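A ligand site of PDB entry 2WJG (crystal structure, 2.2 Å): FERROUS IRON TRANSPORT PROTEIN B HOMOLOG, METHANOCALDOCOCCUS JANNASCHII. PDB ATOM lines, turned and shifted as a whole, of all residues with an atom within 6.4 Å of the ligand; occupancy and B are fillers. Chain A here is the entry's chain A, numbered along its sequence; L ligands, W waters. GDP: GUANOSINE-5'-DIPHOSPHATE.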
ATOM      1  N   GLY A  14     -15.744  18.479 -12.952  1.00  0.00           N
ATOM      2  CA  GLY A  14     -15.369  19.760 -13.534  1.00  0.00           C
ATOM      3  C   GLY A  14     -15.271  20.844 -12.486  1.00  0.00           C
ATOM      4  O   GLY A  14     -15.461  20.585 -11.289  1.00  0.00           O
ATOM      5  N   ASN A  15     -14.958  22.068 -12.919  1.00  0.00           N
ATOM      6  CA  ASN A  15     -15.071  23.251 -12.071  1.00  0.00           C
ATOM      7  C   ASN A  15     -16.494  23.333 -11.529  1.00  0.00           C
ATOM      8  O   ASN A  15     -17.409  22.749 -12.095  1.00  0.00           O
ATOM      9  CB  ASN A  15     -14.817  24.531 -12.864  1.00  0.00           C
ATOM     10  CG  ASN A  15     -13.435  24.595 -13.502  1.00  0.00           C
ATOM     11  OD1 ASN A  15     -13.085  25.591 -14.146  1.00  0.00           O
ATOM     12  ND2 ASN A  15     -12.648  23.538 -13.338  1.00  0.00           N
ATOM     13  N   PRO A  16     -16.679  24.086 -10.431  1.00  0.00           N
ATOM     14  CA  PRO A  16     -18.027  24.347  -9.928  1.00  0.00           C
ATOM     15  C   PRO A  16     -18.809  25.180 -10.923  1.00  0.00           C
ATOM     16  O   PRO A  16     -18.211  25.930 -11.685  1.00  0.00           O
ATOM     17  CB  PRO A  16     -17.773  25.165  -8.661  1.00  0.00           C
ATOM     18  CG  PRO A  16     -16.363  24.729  -8.215  1.00  0.00           C
ATOM     19  CD  PRO A  16     -15.634  24.576  -9.515  1.00  0.00           C
ATOM     20  N   ASN A  17     -20.138  25.050 -10.906  1.00  0.00           N
ATOM     21  CA  ASN A  17     -20.994  25.923 -11.695  1.00  0.00           C
ATOM     22  C   ASN A  17     -20.866  25.764 -13.202  1.00  0.00           C
ATOM     23  O   ASN A  17     -21.139  26.710 -13.947  1.00  0.00           O
ATOM     24  CB  ASN A  17     -20.732  27.387 -11.333  1.00  0.00           C
ATOM     25  CG  ASN A  17     -21.984  28.232 -11.365  1.00  0.00           C
ATOM     26  OD1 ASN A  17     -23.007  27.870 -10.764  1.00  0.00           O
ATOM     27  ND2 ASN A  17     -21.913  29.374 -12.053  1.00  0.00           N
ATOM     28  N   VAL A  18     -20.436  24.603 -13.678  1.00  0.00           N
ATOM     29  CA  VAL A  18     -20.310  24.412 -15.128  1.00  0.00           C
ATOM     30  C   VAL A  18     -21.472  23.650 -15.751  1.00  0.00           C
ATOM     31  O   VAL A  18     -21.487  23.472 -16.955  1.00  0.00           O
ATOM     32  CB  VAL A  18     -19.013  23.646 -15.492  1.00  0.00           C
ATOM     33  CG1 VAL A  18     -17.784  24.404 -15.033  1.00  0.00           C
ATOM     34  CG2 VAL A  18     -19.049  22.247 -14.882  1.00  0.00           C
ATOM     35  N   GLY A  19     -22.407  23.153 -14.940  1.00  0.00           N
ATOM     36  CA  GLY A  19     -23.530  22.377 -15.442  1.00  0.00           C
ATOM     37  C   GLY A  19     -23.499  20.894 -15.099  1.00  0.00           C
ATOM     38  O   GLY A  19     -24.219  20.076 -15.662  1.00  0.00           O
ATOM     39  N   LYS A  20     -22.652  20.558 -14.156  1.00  0.00           N
ATOM     40  CA  LYS A  20     -22.468  19.180 -13.724  1.00  0.00           C
ATOM     41  C   LYS A  20     -23.763  18.586 -13.160  1.00  0.00           C
ATOM     42  O   LYS A  20     -24.155  17.468 -13.503  1.00  0.00           O
ATOM     43  CB  LYS A  20     -21.383  19.186 -12.644  1.00  0.00           C
ATOM     44  CG  LYS A  20     -20.469  17.995 -12.641  1.00  0.00           C
ATOM     45  CD  LYS A  20     -18.999  18.438 -12.465  1.00  0.00           C
ATOM     46  CE  LYS A  20     -18.712  19.269 -11.188  1.00  0.00           C
ATOM     47  NZ  LYS A  20     -19.376  20.618 -11.022  1.00  0.00           N
ATOM     48  N   SER A  21     -24.420  19.328 -12.279  1.00  0.00           N
ATOM     49  CA  SER A  21     -25.662  18.870 -11.706  1.00  0.00           C
ATOM     50  C   SER A  21     -26.726  18.754 -12.797  1.00  0.00           C
ATOM     51  O   SER A  21     -27.468  17.768 -12.885  1.00  0.00           O
ATOM     52  CB  SER A  21     -26.114  19.854 -10.639  1.00  0.00           C
ATOM     53  OG  SER A  21     -26.540  19.167  -9.489  1.00  0.00           O
ATOM     54  N   THR A  22     -26.785  19.788 -13.643  1.00  0.00           N
ATOM     55  CA  THR A  22     -27.740  19.824 -14.739  1.00  0.00           C
ATOM     56  C   THR A  22     -27.572  18.621 -15.650  1.00  0.00           C
ATOM     57  O   THR A  22     -28.539  17.962 -16.037  1.00  0.00           O
ATOM     58  CB  THR A  22     -27.559  21.114 -15.539  1.00  0.00           C
ATOM     59  OG1 THR A  22     -27.659  22.222 -14.628  1.00  0.00           O
ATOM     60  CG2 THR A  22     -28.626  21.246 -16.631  1.00  0.00           C
ATOM     61  N   ILE A  23     -26.319  18.321 -15.981  1.00  0.00           N
ATOM     62  CA  ILE A  23     -26.024  17.168 -16.814  1.00  0.00           C
ATOM     63  C   ILE A  23     -26.317  15.861 -16.088  1.00  0.00           C
ATOM     64  O   ILE A  23     -26.879  14.932 -16.678  1.00  0.00           O
ATOM     65  CB  ILE A  23     -24.597  17.216 -17.355  1.00  0.00           C
ATOM     66  CG1 ILE A  23     -24.488  18.324 -18.403  1.00  0.00           C
ATOM     67  CG2 ILE A  23     -24.207  15.890 -17.992  1.00  0.00           C
ATOM     68  CD1 ILE A  23     -23.090  18.597 -18.863  1.00  0.00           C
ATOM     69  N   LYS A  45     -23.577  12.530  -5.161  1.00  0.00           N
ATOM     70  CA  LYS A  45     -24.717  12.078  -5.967  1.00  0.00           C
ATOM     71  C   LYS A  45     -24.334  10.918  -6.883  1.00  0.00           C
ATOM     72  O   LYS A  45     -23.342  10.991  -7.600  1.00  0.00           O
ATOM     73  CB  LYS A  45     -25.283  13.210  -6.840  1.00  0.00           C
ATOM     74  CG  LYS A  45     -25.988  14.330  -6.099  1.00  0.00           C
ATOM     75  CD  LYS A  45     -26.904  15.108  -7.046  1.00  0.00           C
ATOM     76  CE  LYS A  45     -26.143  16.143  -7.851  1.00  0.00           C
ATOM     77  NZ  LYS A  45     -26.273  17.502  -7.256  1.00  0.00           N
ATOM     78  N   ASP A  60     -21.313  11.712  -9.426  1.00  0.00           N
ATOM     79  CA  ASP A  60     -20.942  13.111  -9.537  1.00  0.00           C
ATOM     80  C   ASP A  60     -19.813  13.387  -8.552  1.00  0.00           C
ATOM     81  O   ASP A  60     -19.978  13.260  -7.347  1.00  0.00           O
ATOM     82  CB  ASP A  60     -22.135  14.012  -9.222  1.00  0.00           C
ATOM     83  CG  ASP A  60     -21.904  15.442  -9.637  1.00  0.00           C
ATOM     84  OD1 ASP A  60     -20.885  15.673 -10.299  1.00  0.00           O
ATOM     85  OD2 ASP A  60     -22.723  16.346  -9.342  1.00  0.00           O
ATOM     86  N   ILE A  92     -16.591  17.805 -17.545  1.00  0.00           N
ATOM     87  CA  ILE A  92     -17.544  18.797 -18.001  1.00  0.00           C
ATOM     88  C   ILE A  92     -16.903  20.171 -17.904  1.00  0.00           C
ATOM     89  O   ILE A  92     -16.504  20.609 -16.825  1.00  0.00           O
ATOM     90  CB  ILE A  92     -18.826  18.772 -17.182  1.00  0.00           C
ATOM     91  CG1 ILE A  92     -19.487  17.396 -17.316  1.00  0.00           C
ATOM     92  CG2 ILE A  92     -19.787  19.851 -17.674  1.00  0.00           C
ATOM     93  CD1 ILE A  92     -20.603  17.207 -16.347  1.00  0.00           C
ATOM     94  N   ASN A 120     -19.940  22.264 -22.301  1.00  0.00           N
ATOM     95  CA  ASN A 120     -21.276  22.738 -21.956  1.00  0.00           C
ATOM     96  C   ASN A 120     -21.398  24.236 -22.093  1.00  0.00           C
ATOM     97  O   ASN A 120     -20.398  24.931 -22.259  1.00  0.00           O
ATOM     98  CB  ASN A 120     -21.623  22.304 -20.511  1.00  0.00           C
ATOM     99  CG  ASN A 120     -23.108  22.424 -20.193  1.00  0.00           C
ATOM    100  OD1 ASN A 120     -23.506  22.736 -19.066  1.00  0.00           O
ATOM    101  ND2 ASN A 120     -23.940  22.180 -21.199  1.00  0.00           N
ATOM    102  N   LYS A 121     -22.624  24.742 -22.014  1.00  0.00           N
ATOM    103  CA  LYS A 121     -22.900  26.180 -22.125  1.00  0.00           C
ATOM    104  C   LYS A 121     -22.574  26.796 -23.489  1.00  0.00           C
ATOM    105  O   LYS A 121     -22.268  28.005 -23.589  1.00  0.00           O
ATOM    106  CB  LYS A 121     -22.203  26.942 -20.979  1.00  0.00           C
ATOM    107  CG  LYS A 121     -22.653  26.487 -19.588  1.00  0.00           C
ATOM    108  CD  LYS A 121     -22.482  27.566 -18.546  1.00  0.00           C
ATOM    109  CE  LYS A 121     -22.749  27.018 -17.162  1.00  0.00           C
ATOM    110  NZ  LYS A 121     -22.624  28.077 -16.147  1.00  0.00           N
ATOM    111  N   MET A 122     -22.659  25.990 -24.552  1.00  0.00           N
ATOM    112  CA  MET A 122     -22.438  26.512 -25.920  1.00  0.00           C
ATOM    113  C   MET A 122     -23.377  27.690 -26.198  1.00  0.00           C
ATOM    114  O   MET A 122     -22.993  28.662 -26.852  1.00  0.00           O
ATOM    115  CB  MET A 122     -22.636  25.423 -26.979  1.00  0.00           C
ATOM    116  CG  MET A 122     -21.645  24.280 -26.888  1.00  0.00           C
ATOM    117  SD  MET A 122     -20.003  24.897 -27.187  1.00  0.00           S
ATOM    118  CE  MET A 122     -20.056  25.135 -28.986  1.00  0.00           C
ATOM    119  N   ASP A 123     -24.606  27.588 -25.703  1.00  0.00           N
ATOM    120  CA  ASP A 123     -25.577  28.666 -25.901  1.00  0.00           C
ATOM    121  C   ASP A 123     -25.095  29.944 -25.242  1.00  0.00           C
ATOM    122  O   ASP A 123     -25.185  31.022 -25.839  1.00  0.00           O
ATOM    123  CB  ASP A 123     -26.968  28.279 -25.392  1.00  0.00           C
ATOM    124  CG  ASP A 123     -27.017  28.170 -23.880  1.00  0.00           C
ATOM    125  OD1 ASP A 123     -27.904  28.810 -23.254  1.00  0.00           O
ATOM    126  OD2 ASP A 123     -26.161  27.461 -23.303  1.00  0.00           O
ATOM    127  N   LEU A 124     -24.583  29.851 -24.013  1.00  0.00           N
ATOM    128  CA  LEU A 124     -24.120  31.037 -23.289  1.00  0.00           C
ATOM    129  C   LEU A 124     -22.944  31.658 -24.017  1.00  0.00           C
ATOM    130  O   LEU A 124     -22.849  32.883 -24.122  1.00  0.00           O
ATOM    131  CB  LEU A 124     -23.708  30.698 -21.855  1.00  0.00           C
ATOM    132  CG  LEU A 124     -24.047  31.693 -20.730  1.00  0.00           C
ATOM    133  CD1 LEU A 124     -22.948  31.701 -19.710  1.00  0.00           C
ATOM    134  CD2 LEU A 124     -24.303  33.113 -21.225  1.00  0.00           C
ATOM    135  N   LEU A 148     -22.587  20.914 -26.104  1.00  0.00           N
ATOM    136  CA  LEU A 148     -23.986  20.840 -25.686  1.00  0.00           C
ATOM    137  C   LEU A 148     -24.397  22.077 -24.906  1.00  0.00           C
ATOM    138  O   LEU A 148     -23.557  22.916 -24.515  1.00  0.00           O
ATOM    139  CB  LEU A 148     -24.258  19.575 -24.856  1.00  0.00           C
ATOM    140  CG  LEU A 148     -23.770  19.447 -23.398  1.00  0.00           C
ATOM    141  CD1 LEU A 148     -24.602  18.409 -22.650  1.00  0.00           C
ATOM    142  CD2 LEU A 148     -22.315  19.054 -23.338  1.00  0.00           C
ATOM    143  N   SER A 149     -25.710  22.201 -24.687  1.00  0.00           N
ATOM    144  CA  SER A 149     -26.251  23.171 -23.747  1.00  0.00           C
ATOM    145  C   SER A 149     -27.268  22.419 -22.901  1.00  0.00           C
ATOM    146  O   SER A 149     -28.453  22.344 -23.256  1.00  0.00           O
ATOM    147  CB  SER A 149     -26.885  24.351 -24.462  1.00  0.00           C
ATOM    148  OG  SER A 149     -25.928  24.994 -25.305  1.00  0.00           O
ATOM    149  N   ALA A 150     -26.795  21.853 -21.793  1.00  0.00           N
ATOM    150  CA  ALA A 150     -27.635  20.969 -20.997  1.00  0.00           C
ATOM    151  C   ALA A 150     -28.874  21.680 -20.453  1.00  0.00           C
ATOM    152  O   ALA A 150     -29.924  21.060 -20.280  1.00  0.00           O
ATOM    153  CB  ALA A 150     -26.845  20.355 -19.857  1.00  0.00           C
ATOM    154  N   ALA A 151     -28.751  22.970 -20.160  1.00  0.00           N
ATOM    155  CA  ALA A 151     -29.857  23.658 -19.512  1.00  0.00           C
ATOM    156  C   ALA A 151     -30.985  23.843 -20.514  1.00  0.00           C
ATOM    157  O   ALA A 151     -32.139  23.962 -20.140  1.00  0.00           O
ATOM    158  CB  ALA A 151     -29.393  24.999 -18.943  1.00  0.00           C
ATOM    159  N   LYS A 152     -30.622  23.840 -21.792  1.00  0.00           N
ATOM    160  CA  LYS A 152     -31.579  24.033 -22.876  1.00  0.00           C
ATOM    161  C   LYS A 152     -31.916  22.676 -23.481  1.00  0.00           C
ATOM    162  O   LYS A 152     -32.625  22.582 -24.480  1.00  0.00           O
ATOM    163  CB  LYS A 152     -31.009  25.024 -23.896  1.00  0.00           C
ATOM    164  CG  LYS A 152     -31.314  24.752 -25.350  1.00  0.00           C
ATOM    165  CD  LYS A 152     -30.445  25.602 -26.302  1.00  0.00           C
ATOM    166  CE  LYS A 152     -31.133  26.909 -26.744  1.00  0.00           C
ATOM    167  NZ  LYS A 152     -31.052  28.005 -25.736  1.00  0.00           N
HETATM  168  PB  GDP L   1     -22.580  22.665 -11.217  1.00  0.00           P
HETATM  169  O1B GDP L   1     -23.167  21.365 -10.690  1.00  0.00           O
HETATM  170  O2B GDP L   1     -21.367  22.330 -12.062  1.00  0.00           O
HETATM  171  O3B GDP L   1     -22.175  23.530 -10.032  1.00  0.00           O
HETATM  172  O3A GDP L   1     -23.553  23.519 -12.164  1.00  0.00           O
HETATM  173  PA  GDP L   1     -25.163  23.432 -12.174  1.00  0.00           P
HETATM  174  O1A GDP L   1     -25.843  23.628 -10.847  1.00  0.00           O
HETATM  175  O2A GDP L   1     -25.589  22.123 -12.810  1.00  0.00           O
HETATM  176  O5' GDP L   1     -25.432  24.709 -13.111  1.00  0.00           O
HETATM  177  C5' GDP L   1     -25.015  25.993 -12.619  1.00  0.00           C
HETATM  178  C4' GDP L   1     -25.787  27.071 -13.363  1.00  0.00           C
HETATM  179  O4' GDP L   1     -25.484  27.004 -14.765  1.00  0.00           O
HETATM  180  C3' GDP L   1     -27.272  26.812 -13.224  1.00  0.00           C
HETATM  181  O3' GDP L   1     -27.887  28.087 -13.065  1.00  0.00           O
HETATM  182  C2' GDP L   1     -27.669  26.182 -14.544  1.00  0.00           C
HETATM  183  O2' GDP L   1     -29.009  26.472 -14.940  1.00  0.00           O
HETATM  184  C1' GDP L   1     -26.713  26.871 -15.483  1.00  0.00           C
HETATM  185  N9  GDP L   1     -26.511  26.035 -16.671  1.00  0.00           N
HETATM  186  C8  GDP L   1     -26.290  24.705 -16.706  1.00  0.00           C
HETATM  187  N7  GDP L   1     -26.131  24.297 -17.988  1.00  0.00           N
HETATM  188  C5  GDP L   1     -26.250  25.380 -18.791  1.00  0.00           C
HETATM  189  C6  GDP L   1     -26.209  25.643 -20.256  1.00  0.00           C
HETATM  190  O6  GDP L   1     -25.999  24.709 -21.081  1.00  0.00           O
HETATM  191  N1  GDP L   1     -26.394  26.913 -20.658  1.00  0.00           N
HETATM  192  C2  GDP L   1     -26.612  27.920 -19.769  1.00  0.00           C
HETATM  193  N2  GDP L   1     -26.772  29.173 -20.231  1.00  0.00           N
HETATM  194  N3  GDP L   1     -26.676  27.751 -18.427  1.00  0.00           N
HETATM  195  C4  GDP L   1     -26.491  26.512 -17.901  1.00  0.00           C
HETATM  196  O   HOH W   1     -25.318  29.758 -16.615  1.00  0.00           O
HETATM  197  O   HOH W   2     -22.347  19.247  -9.356  1.00  0.00           O
HETATM  198  O   HOH W   3     -26.103  29.643 -10.657  1.00  0.00           O
HETATM  199  O   HOH W   4     -30.013  28.886 -16.293  1.00  0.00           O
HETATM  200  O   HOH W   5     -30.187  28.263 -12.025  1.00  0.00           O
HETATM  201  O   HOH W   6     -28.356  23.001 -10.207  1.00  0.00           O
HETATM  202  O   HOH W   7     -26.543  30.377 -13.654  1.00  0.00           O
HETATM  203  O   HOH W   8     -23.422  25.838  -9.064  1.00  0.00           O
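OD1 of Asn 120 lies close to N7 of the ligand, at 3.2 Å. The backbone NH of Val 18 is in hydrogen-bond range of an oxygen (O2B) of the ligand (2.9 Å). OD2 of Asp 123 is in hydrogen-bond range of N1 of the ligand (2.7 Å). O3B of the ligand lies within hydrogen-bond range of N of Asn 17 (2.7 Å). The side-chain hydroxyl of Thr 22 lies within hydrogen-bond range of an oxygen (O2A) of the ligand. The side-chain amino group of Lys 121 lies within hydrogen-bond range of an oxygen (O4') of the ligand (3.4 Å). The backbone NH (N) of Ala 151 is in hydrogen-bond range of an oxygen (O6) of the ligand, 3.4 Å away. The backbone NH (N) of Gly 19 sits at hydrogen-bond distance from an oxygen (O3A) of the ligand (3.0 Å). The backbone NH of Thr 22 lies within hydrogen-bond range of an oxygen (O2A) of the ligand (2.8 Å). An oxygen (O6) of the ligand sits at hydrogen-bond distance from the backbone NH (N) of Ala 150, 3.0 Å away. N of Lys 20 lies within hydrogen-bond range of O2B of the ligand, at 3.0 Å. O1B of the ligand sits at hydrogen-bond distance from N of Ser 21. The side-chain amino group (NZ) of Lys 20 is in salt-bridge range of an oxygen (O2B) of the ligand (2.8 Å).
Water W2 bridges O1B of the ligand (2.6 Å) and OD2 of Asp 60 (2.9 Å). Water W8 lies within hydrogen-bond range of OD1 of Asn 17 (2.7 Å) and O3B of the ligand (2.8 Å). Water W1 lies within hydrogen-bond range of N3 of the ligand and NZ of Lys 121.
Asn 15 touches the ligand (O to O2B, 3.98 Å). C of Pro 16 touches O3B of the ligand (3.9 Å). Leu 124 touches the ligand (CG to N2, 3.7 Å). CA of Ser 149 touches O6 of the ligand, 3.1 Å away. Of the 23 residues printed, 15 come within 4 Å of the ligand.
NZ of Lys 20 lies within hydrogen-bond range of O of Asn 15 (3.1 Å). O of Leu 148 is in hydrogen-bond range of N of Lys 121, at 3.2 Å. The side-chain amide nitrogen of Asn 120 sits at hydrogen-bond distance from the backbone carbonyl oxygen of Leu 148, at 3.4 Å. NZ of Lys 121 lies within hydrogen-bond range of O of Asn 17, at 3.0 Å. OG of Ser 149 is in hydrogen-bond range of N of Met 122, 3.5 Å away. N of Ala 150 sits close to ND2 of Asn 120. N of Asp 123 is in hydrogen-bond range of OG of Ser 149. The side-chain amino group (NZ) of Lys 45 is in hydrogen-bond range of the side-chain hydroxyl (OG) of Ser 21 (2.8 Å).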
